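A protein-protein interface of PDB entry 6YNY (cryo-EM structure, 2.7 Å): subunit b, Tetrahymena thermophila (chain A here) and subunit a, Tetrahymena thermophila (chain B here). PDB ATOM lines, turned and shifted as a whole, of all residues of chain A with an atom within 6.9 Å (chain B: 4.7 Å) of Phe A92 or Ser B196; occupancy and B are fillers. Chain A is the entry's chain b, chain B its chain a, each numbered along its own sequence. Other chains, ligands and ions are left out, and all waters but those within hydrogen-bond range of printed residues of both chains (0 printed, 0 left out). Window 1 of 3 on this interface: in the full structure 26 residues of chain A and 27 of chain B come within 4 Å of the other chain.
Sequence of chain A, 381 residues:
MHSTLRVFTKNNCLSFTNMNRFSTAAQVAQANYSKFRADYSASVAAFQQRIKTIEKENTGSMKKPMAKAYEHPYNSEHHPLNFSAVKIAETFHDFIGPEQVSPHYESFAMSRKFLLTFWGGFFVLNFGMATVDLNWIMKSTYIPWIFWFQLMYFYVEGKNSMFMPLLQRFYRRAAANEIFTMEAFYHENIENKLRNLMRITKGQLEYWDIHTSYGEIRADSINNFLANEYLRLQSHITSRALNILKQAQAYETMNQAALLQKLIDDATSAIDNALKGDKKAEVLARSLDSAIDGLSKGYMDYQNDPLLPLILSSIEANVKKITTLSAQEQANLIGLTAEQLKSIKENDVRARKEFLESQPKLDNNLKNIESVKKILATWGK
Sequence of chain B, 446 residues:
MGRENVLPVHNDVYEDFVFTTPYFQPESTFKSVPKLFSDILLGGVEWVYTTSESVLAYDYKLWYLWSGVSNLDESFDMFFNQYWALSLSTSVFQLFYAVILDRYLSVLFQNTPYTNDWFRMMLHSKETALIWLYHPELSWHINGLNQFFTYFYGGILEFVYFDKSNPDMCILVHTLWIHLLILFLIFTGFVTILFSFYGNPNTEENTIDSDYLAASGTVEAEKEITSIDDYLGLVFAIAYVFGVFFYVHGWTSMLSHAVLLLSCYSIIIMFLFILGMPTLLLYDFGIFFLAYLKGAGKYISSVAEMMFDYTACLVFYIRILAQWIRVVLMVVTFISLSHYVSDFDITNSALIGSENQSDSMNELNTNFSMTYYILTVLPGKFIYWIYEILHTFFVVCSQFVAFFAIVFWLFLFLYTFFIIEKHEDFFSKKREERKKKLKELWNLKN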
ATOM      1  N   LYS A  87      19.058   6.732 -23.520  1.00  0.00           N
ATOM      2  CA  LYS A  87      20.342   6.157 -23.893  1.00  0.00           C
ATOM      3  C   LYS A  87      20.242   4.650 -24.067  1.00  0.00           C
ATOM      4  O   LYS A  87      20.928   4.080 -24.921  1.00  0.00           O
ATOM      5  CB  LYS A  87      21.398   6.505 -22.847  1.00  0.00           C
ATOM      6  CG  LYS A  87      22.786   6.019 -23.179  1.00  0.00           C
ATOM      7  CD  LYS A  87      23.286   6.619 -24.472  1.00  0.00           C
ATOM      8  CE  LYS A  87      24.661   6.119 -24.821  1.00  0.00           C
ATOM      9  NZ  LYS A  87      25.157   6.765 -26.056  1.00  0.00           N
ATOM     10  N   ILE A  88      19.402   3.991 -23.270  1.00  0.00           N
ATOM     11  CA  ILE A  88      19.184   2.563 -23.445  1.00  0.00           C
ATOM     12  C   ILE A  88      18.538   2.290 -24.792  1.00  0.00           C
ATOM     13  O   ILE A  88      18.787   1.250 -25.412  1.00  0.00           O
ATOM     14  CB  ILE A  88      18.333   2.006 -22.289  1.00  0.00           C
ATOM     15  CG1 ILE A  88      19.019   2.270 -20.954  1.00  0.00           C
ATOM     16  CG2 ILE A  88      18.111   0.525 -22.467  1.00  0.00           C
ATOM     17  CD1 ILE A  88      18.188   1.910 -19.765  1.00  0.00           C
ATOM     18  N   ALA A  89      17.700   3.211 -25.270  1.00  0.00           N
ATOM     19  CA  ALA A  89      17.088   3.046 -26.581  1.00  0.00           C
ATOM     20  C   ALA A  89      18.127   3.136 -27.688  1.00  0.00           C
ATOM     21  O   ALA A  89      18.067   2.382 -28.665  1.00  0.00           O
ATOM     22  CB  ALA A  89      16.001   4.096 -26.782  1.00  0.00           C
ATOM     23  N   GLU A  90      19.080   4.055 -27.555  1.00  0.00           N
ATOM     24  CA  GLU A  90      20.144   4.168 -28.542  1.00  0.00           C
ATOM     25  C   GLU A  90      20.988   2.902 -28.583  1.00  0.00           C
ATOM     26  O   GLU A  90      21.308   2.389 -29.661  1.00  0.00           O
ATOM     27  CB  GLU A  90      21.009   5.384 -28.224  1.00  0.00           C
ATOM     28  CG  GLU A  90      22.010   5.732 -29.296  1.00  0.00           C
ATOM     29  CD  GLU A  90      22.932   6.854 -28.884  1.00  0.00           C
ATOM     30  OE1 GLU A  90      24.151   6.745 -29.133  1.00  0.00           O
ATOM     31  OE2 GLU A  90      22.442   7.842 -28.303  1.00  0.00           O
ATOM     32  N   THR A  91      21.359   2.381 -27.413  1.00  0.00           N
ATOM     33  CA  THR A  91      22.143   1.153 -27.368  1.00  0.00           C
ATOM     34  C   THR A  91      21.344  -0.038 -27.871  1.00  0.00           C
ATOM     35  O   THR A  91      21.920  -0.988 -28.412  1.00  0.00           O
ATOM     36  CB  THR A  91      22.629   0.887 -25.946  1.00  0.00           C
ATOM     37  OG1 THR A  91      21.506   0.724 -25.074  1.00  0.00           O
ATOM     38  CG2 THR A  91      23.476   2.026 -25.448  1.00  0.00           C
ATOM     39  N   PHE A  92      20.023  -0.008 -27.704  1.00  0.00           N
ATOM     40  CA  PHE A  92      19.197  -1.125 -28.142  1.00  0.00           C
ATOM     41  C   PHE A  92      19.086  -1.161 -29.659  1.00  0.00           C
ATOM     42  O   PHE A  92      19.306  -2.205 -30.281  1.00  0.00           O
ATOM     43  CB  PHE A  92      17.820  -1.028 -27.494  1.00  0.00           C
ATOM     44  CG  PHE A  92      16.859  -2.072 -27.958  1.00  0.00           C
ATOM     45  CD1 PHE A  92      15.797  -1.737 -28.769  1.00  0.00           C
ATOM     46  CD2 PHE A  92      17.018  -3.389 -27.590  1.00  0.00           C
ATOM     47  CE1 PHE A  92      14.915  -2.690 -29.195  1.00  0.00           C
ATOM     48  CE2 PHE A  92      16.136  -4.347 -28.017  1.00  0.00           C
ATOM     49  CZ  PHE A  92      15.083  -3.997 -28.821  1.00  0.00           C
ATOM     50  N   HIS A  93      18.755  -0.027 -30.274  1.00  0.00           N
ATOM     51  CA  HIS A  93      18.617   0.016 -31.722  1.00  0.00           C
ATOM     52  C   HIS A  93      19.953  -0.130 -32.432  1.00  0.00           C
ATOM     53  O   HIS A  93      19.975  -0.473 -33.618  1.00  0.00           O
ATOM     54  CB  HIS A  93      17.926   1.306 -32.147  1.00  0.00           C
ATOM     55  CG  HIS A  93      16.469   1.338 -31.814  1.00  0.00           C
ATOM     56  ND1 HIS A  93      15.972   1.989 -30.708  1.00  0.00           N
ATOM     57  CD2 HIS A  93      15.404   0.779 -32.434  1.00  0.00           C
ATOM     58  CE1 HIS A  93      14.660   1.840 -30.666  1.00  0.00           C
ATOM     59  NE2 HIS A  93      14.290   1.109 -31.701  1.00  0.00           N
ATOM     60  N   ASP A  94      21.062   0.122 -31.742  1.00  0.00           N
ATOM     61  CA  ASP A  94      22.359  -0.207 -32.312  1.00  0.00           C
ATOM     62  C   ASP A  94      22.604  -1.708 -32.291  1.00  0.00           C
ATOM     63  O   ASP A  94      23.357  -2.225 -33.122  1.00  0.00           O
ATOM     64  CB  ASP A  94      23.464   0.518 -31.552  1.00  0.00           C
ATOM     65  CG  ASP A  94      23.371   2.022 -31.683  1.00  0.00           C
ATOM     66  OD1 ASP A  94      22.415   2.505 -32.323  1.00  0.00           O
ATOM     67  OD2 ASP A  94      24.252   2.723 -31.146  1.00  0.00           O
ATOM     68  N   PHE A  95      21.974  -2.417 -31.356  1.00  0.00           N
ATOM     69  CA  PHE A  95      22.133  -3.861 -31.254  1.00  0.00           C
ATOM     70  C   PHE A  95      21.278  -4.592 -32.283  1.00  0.00           C
ATOM     71  O   PHE A  95      21.788  -5.397 -33.069  1.00  0.00           O
ATOM     72  CB  PHE A  95      21.793  -4.308 -29.832  1.00  0.00           C
ATOM     73  CG  PHE A  95      21.456  -5.760 -29.709  1.00  0.00           C
ATOM     74  CD1 PHE A  95      20.257  -6.150 -29.153  1.00  0.00           C
ATOM     75  CD2 PHE A  95      22.329  -6.734 -30.146  1.00  0.00           C
ATOM     76  CE1 PHE A  95      19.937  -7.472 -29.034  1.00  0.00           C
ATOM     77  CE2 PHE A  95      22.011  -8.059 -30.032  1.00  0.00           C
ATOM     78  CZ  PHE A  95      20.813  -8.431 -29.476  1.00  0.00           C
ATOM     79  N   ILE A  96      19.970  -4.332 -32.289  1.00  0.00           N
ATOM     80  CA  ILE A  96      19.098  -4.953 -33.277  1.00  0.00           C
ATOM     81  C   ILE A  96      19.316  -4.395 -34.669  1.00  0.00           C
ATOM     82  O   ILE A  96      18.800  -4.954 -35.641  1.00  0.00           O
ATOM     83  CB  ILE A  96      17.615  -4.788 -32.889  1.00  0.00           C
ATOM     84  CG1 ILE A  96      17.270  -3.314 -32.693  1.00  0.00           C
ATOM     85  CG2 ILE A  96      17.318  -5.575 -31.647  1.00  0.00           C
ATOM     86  CD1 ILE A  96      15.808  -3.048 -32.565  1.00  0.00           C
ATOM     87  N   GLY A  97      20.069  -3.312 -34.788  1.00  0.00           N
ATOM     88  CA  GLY A  97      20.339  -2.711 -36.064  1.00  0.00           C
ATOM     89  C   GLY A  97      19.156  -1.925 -36.577  1.00  0.00           C
ATOM     90  O   GLY A  97      18.055  -1.971 -36.021  1.00  0.00           O
ATOM     91  N   VAL B 191      14.552 -10.436 -23.203  1.00  0.00           N
ATOM     92  CA  VAL B 191      14.427  -9.023 -22.880  1.00  0.00           C
ATOM     93  C   VAL B 191      14.065  -8.218 -24.119  1.00  0.00           C
ATOM     94  O   VAL B 191      13.255  -7.288 -24.056  1.00  0.00           O
ATOM     95  CB  VAL B 191      15.735  -8.527 -22.243  1.00  0.00           C
ATOM     96  CG1 VAL B 191      15.736  -7.028 -22.115  1.00  0.00           C
ATOM     97  CG2 VAL B 191      15.936  -9.175 -20.901  1.00  0.00           C
ATOM     98  N   THR B 192      14.656  -8.561 -25.262  1.00  0.00           N
ATOM     99  CA  THR B 192      14.423  -7.802 -26.481  1.00  0.00           C
ATOM    100  C   THR B 192      12.968  -7.876 -26.921  1.00  0.00           C
ATOM    101  O   THR B 192      12.442  -6.912 -27.486  1.00  0.00           O
ATOM    102  CB  THR B 192      15.343  -8.315 -27.587  1.00  0.00           C
ATOM    103  OG1 THR B 192      16.690  -7.923 -27.309  1.00  0.00           O
ATOM    104  CG2 THR B 192      14.926  -7.784 -28.940  1.00  0.00           C
ATOM    105  N   ILE B 193      12.307  -9.001 -26.675  1.00  0.00           N
ATOM    106  CA  ILE B 193      10.940  -9.198 -27.138  1.00  0.00           C
ATOM    107  C   ILE B 193       9.924  -8.742 -26.101  1.00  0.00           C
ATOM    108  O   ILE B 193       8.914  -8.126 -26.447  1.00  0.00           O
ATOM    109  CB  ILE B 193      10.731 -10.679 -27.510  1.00  0.00           C
ATOM    110  CG1 ILE B 193      11.678 -11.092 -28.634  1.00  0.00           C
ATOM    111  CG2 ILE B 193       9.296 -10.935 -27.904  1.00  0.00           C
ATOM    112  CD1 ILE B 193      11.522 -10.295 -29.902  1.00  0.00           C
ATOM    113  N   LEU B 194      10.168  -9.026 -24.822  1.00  0.00           N
ATOM    114  CA  LEU B 194       9.177  -8.806 -23.781  1.00  0.00           C
ATOM    115  C   LEU B 194       9.473  -7.634 -22.861  1.00  0.00           C
ATOM    116  O   LEU B 194       8.566  -7.191 -22.153  1.00  0.00           O
ATOM    117  CB  LEU B 194       9.026 -10.069 -22.925  1.00  0.00           C
ATOM    118  CG  LEU B 194       8.456 -11.279 -23.653  1.00  0.00           C
ATOM    119  CD1 LEU B 194       8.604 -12.508 -22.803  1.00  0.00           C
ATOM    120  CD2 LEU B 194       7.012 -11.046 -24.001  1.00  0.00           C
ATOM    121  N   PHE B 195      10.698  -7.123 -22.847  1.00  0.00           N
ATOM    122  CA  PHE B 195      11.063  -6.004 -21.989  1.00  0.00           C
ATOM    123  C   PHE B 195      11.820  -4.952 -22.776  1.00  0.00           C
ATOM    124  O   PHE B 195      12.791  -4.364 -22.297  1.00  0.00           O
ATOM    125  CB  PHE B 195      11.873  -6.479 -20.789  1.00  0.00           C
ATOM    126  CG  PHE B 195      11.131  -7.424 -19.901  1.00  0.00           C
ATOM    127  CD1 PHE B 195      10.356  -6.952 -18.864  1.00  0.00           C
ATOM    128  CD2 PHE B 195      11.203  -8.785 -20.107  1.00  0.00           C
ATOM    129  CE1 PHE B 195       9.671  -7.821 -18.050  1.00  0.00           C
ATOM    130  CE2 PHE B 195      10.518  -9.654 -19.294  1.00  0.00           C
ATOM    131  CZ  PHE B 195       9.754  -9.172 -18.267  1.00  0.00           C
ATOM    132  N   SER B 196      11.374  -4.697 -23.998  1.00  0.00           N
ATOM    133  CA  SER B 196      11.915  -3.641 -24.839  1.00  0.00           C
ATOM    134  C   SER B 196      10.842  -2.579 -25.012  1.00  0.00           C
ATOM    135  O   SER B 196       9.781  -2.846 -25.586  1.00  0.00           O
ATOM    136  CB  SER B 196      12.359  -4.191 -26.192  1.00  0.00           C
ATOM    137  OG  SER B 196      11.300  -4.882 -26.829  1.00  0.00           O
ATOM    138  N   PHE B 197      11.123  -1.380 -24.514  1.00  0.00           N
ATOM    139  CA  PHE B 197      10.170  -0.282 -24.530  1.00  0.00           C
ATOM    140  C   PHE B 197      10.782   0.917 -25.231  1.00  0.00           C
ATOM    141  O   PHE B 197      10.713   2.043 -24.732  1.00  0.00           O
ATOM    142  CB  PHE B 197       9.754   0.080 -23.110  1.00  0.00           C
ATOM    143  CG  PHE B 197       9.497  -1.106 -22.240  1.00  0.00           C
ATOM    144  CD1 PHE B 197       8.414  -1.928 -22.475  1.00  0.00           C
ATOM    145  CD2 PHE B 197      10.336  -1.398 -21.189  1.00  0.00           C
ATOM    146  CE1 PHE B 197       8.179  -3.016 -21.680  1.00  0.00           C
ATOM    147  CE2 PHE B 197      10.101  -2.486 -20.390  1.00  0.00           C
ATOM    148  CZ  PHE B 197       9.022  -3.296 -20.635  1.00  0.00           C
ATOM    149  N   TYR B 198      11.387   0.676 -26.389  1.00  0.00           N
ATOM    150  CA  TYR B 198      12.143   1.683 -27.126  1.00  0.00           C
ATOM    151  C   TYR B 198      11.612   1.706 -28.554  1.00  0.00           C
ATOM    152  O   TYR B 198      12.136   1.033 -29.442  1.00  0.00           O
ATOM    153  CB  TYR B 198      13.624   1.369 -27.066  1.00  0.00           C
ATOM    154  CG  TYR B 198      14.032   0.803 -25.732  1.00  0.00           C
ATOM    155  CD1 TYR B 198      13.977   1.574 -24.586  1.00  0.00           C
ATOM    156  CD2 TYR B 198      14.449  -0.509 -25.615  1.00  0.00           C
ATOM    157  CE1 TYR B 198      14.334   1.059 -23.368  1.00  0.00           C
ATOM    158  CE2 TYR B 198      14.810  -1.034 -24.400  1.00  0.00           C
ATOM    159  CZ  TYR B 198      14.751  -0.249 -23.280  1.00  0.00           C
ATOM    160  OH  TYR B 198      15.112  -0.780 -22.068  1.00  0.00           O
ATOM    161  N   GLU B 204       2.839  -0.237 -29.945  1.00  0.00           N
ATOM    162  CA  GLU B 204       3.397  -1.503 -29.490  1.00  0.00           C
ATOM    163  C   GLU B 204       2.678  -1.913 -28.212  1.00  0.00           C
ATOM    164  O   GLU B 204       2.898  -1.326 -27.150  1.00  0.00           O
ATOM    165  CB  GLU B 204       4.902  -1.373 -29.274  1.00  0.00           C
ATOM    166  CG  GLU B 204       5.662  -1.049 -30.544  1.00  0.00           C
ATOM    167  CD  GLU B 204       7.138  -0.820 -30.307  1.00  0.00           C
ATOM    168  OE1 GLU B 204       7.591  -0.984 -29.156  1.00  0.00           O
ATOM    169  OE2 GLU B 204       7.845  -0.473 -31.276  1.00  0.00           O
ATOM    170  N   ASN B 206       3.067  -4.287 -26.282  1.00  0.00           N
ATOM    171  CA  ASN B 206       3.881  -4.847 -25.212  1.00  0.00           C
ATOM    172  C   ASN B 206       4.263  -3.781 -24.194  1.00  0.00           C
ATOM    173  O   ASN B 206       4.250  -4.038 -22.985  1.00  0.00           O
ATOM    174  CB  ASN B 206       5.125  -5.513 -25.792  1.00  0.00           C
ATOM    175  CG  ASN B 206       5.915  -6.268 -24.751  1.00  0.00           C
ATOM    176  OD1 ASN B 206       5.514  -7.344 -24.313  1.00  0.00           O
ATOM    177  ND2 ASN B 206       7.046  -5.714 -24.352  1.00  0.00           N
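The backbone carbonyl oxygen of Tyr B198 sits close to a ring nitrogen (NE2) of His A93.
The backbone NH (N) of Ser B196 sits at hydrogen-bond distance from the backbone carbonyl oxygen (O) of Val B191.
O of Thr B192 is in hydrogen-bond range of OG of Ser B196, at 2.4 Å.
OG1 of Thr A91 sits at hydrogen-bond distance from O of Ile A88.
The backbone carbonyl oxygen (O) of Ala A89 is in hydrogen-bond range of a ring nitrogen (ND1) of His A93 (3.0 Å).
Among the printed residues, merely in contact across the chains: Ile A88 with Tyr B198 (3.3 Å), Ala A89 with Tyr B198 (3.6 Å), Phe A92 with Tyr B198 (3.6 Å), Phe A92 with Thr B192 (3.7 Å), Phe A95 with Thr B192 (3.7 Å) and Phe A92 with Ser B196 (3.8 Å).
Of chain B, only Thr B192 (3.7 Å), Ser B196 (3.8 Å) and Tyr B198 (3.6 Å) come within 4 Å of Phe A92.
Printed residues of chain B within 4 Å of His A93: Tyr B198 (2.9 Å).
Of the printed residues of chain B, Ala A89 touches Tyr B198.
Of the printed residues of chain A, Tyr B198 touches Ile A88, Ala A89, Phe A92 and His A93.
Of the printed residues of chain B, Phe A95 touches Thr B192 (3.7 Å).
Asp A94 touches none of the printed residues of chain B.
The nearest printed residue of chain A that does not touch Ser B196 is Ile A96 (7.3 Å).
Of the 11 printed residues of chain A, 5 touch a printed residue of chain B.
Hydrophobic or aromatic side chains of chain B that line the printed part of chain A: Tyr B198.
Along chain B the printed residues that touch a printed residue of chain A span positions 192 to 198.
Among the printed residues, 7 pairs touch across the chains.
Among the printed residues, no Asp or Glu carboxylate lies within 4 Å of a Lys or Arg side-chain nitrogen of the other chain.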
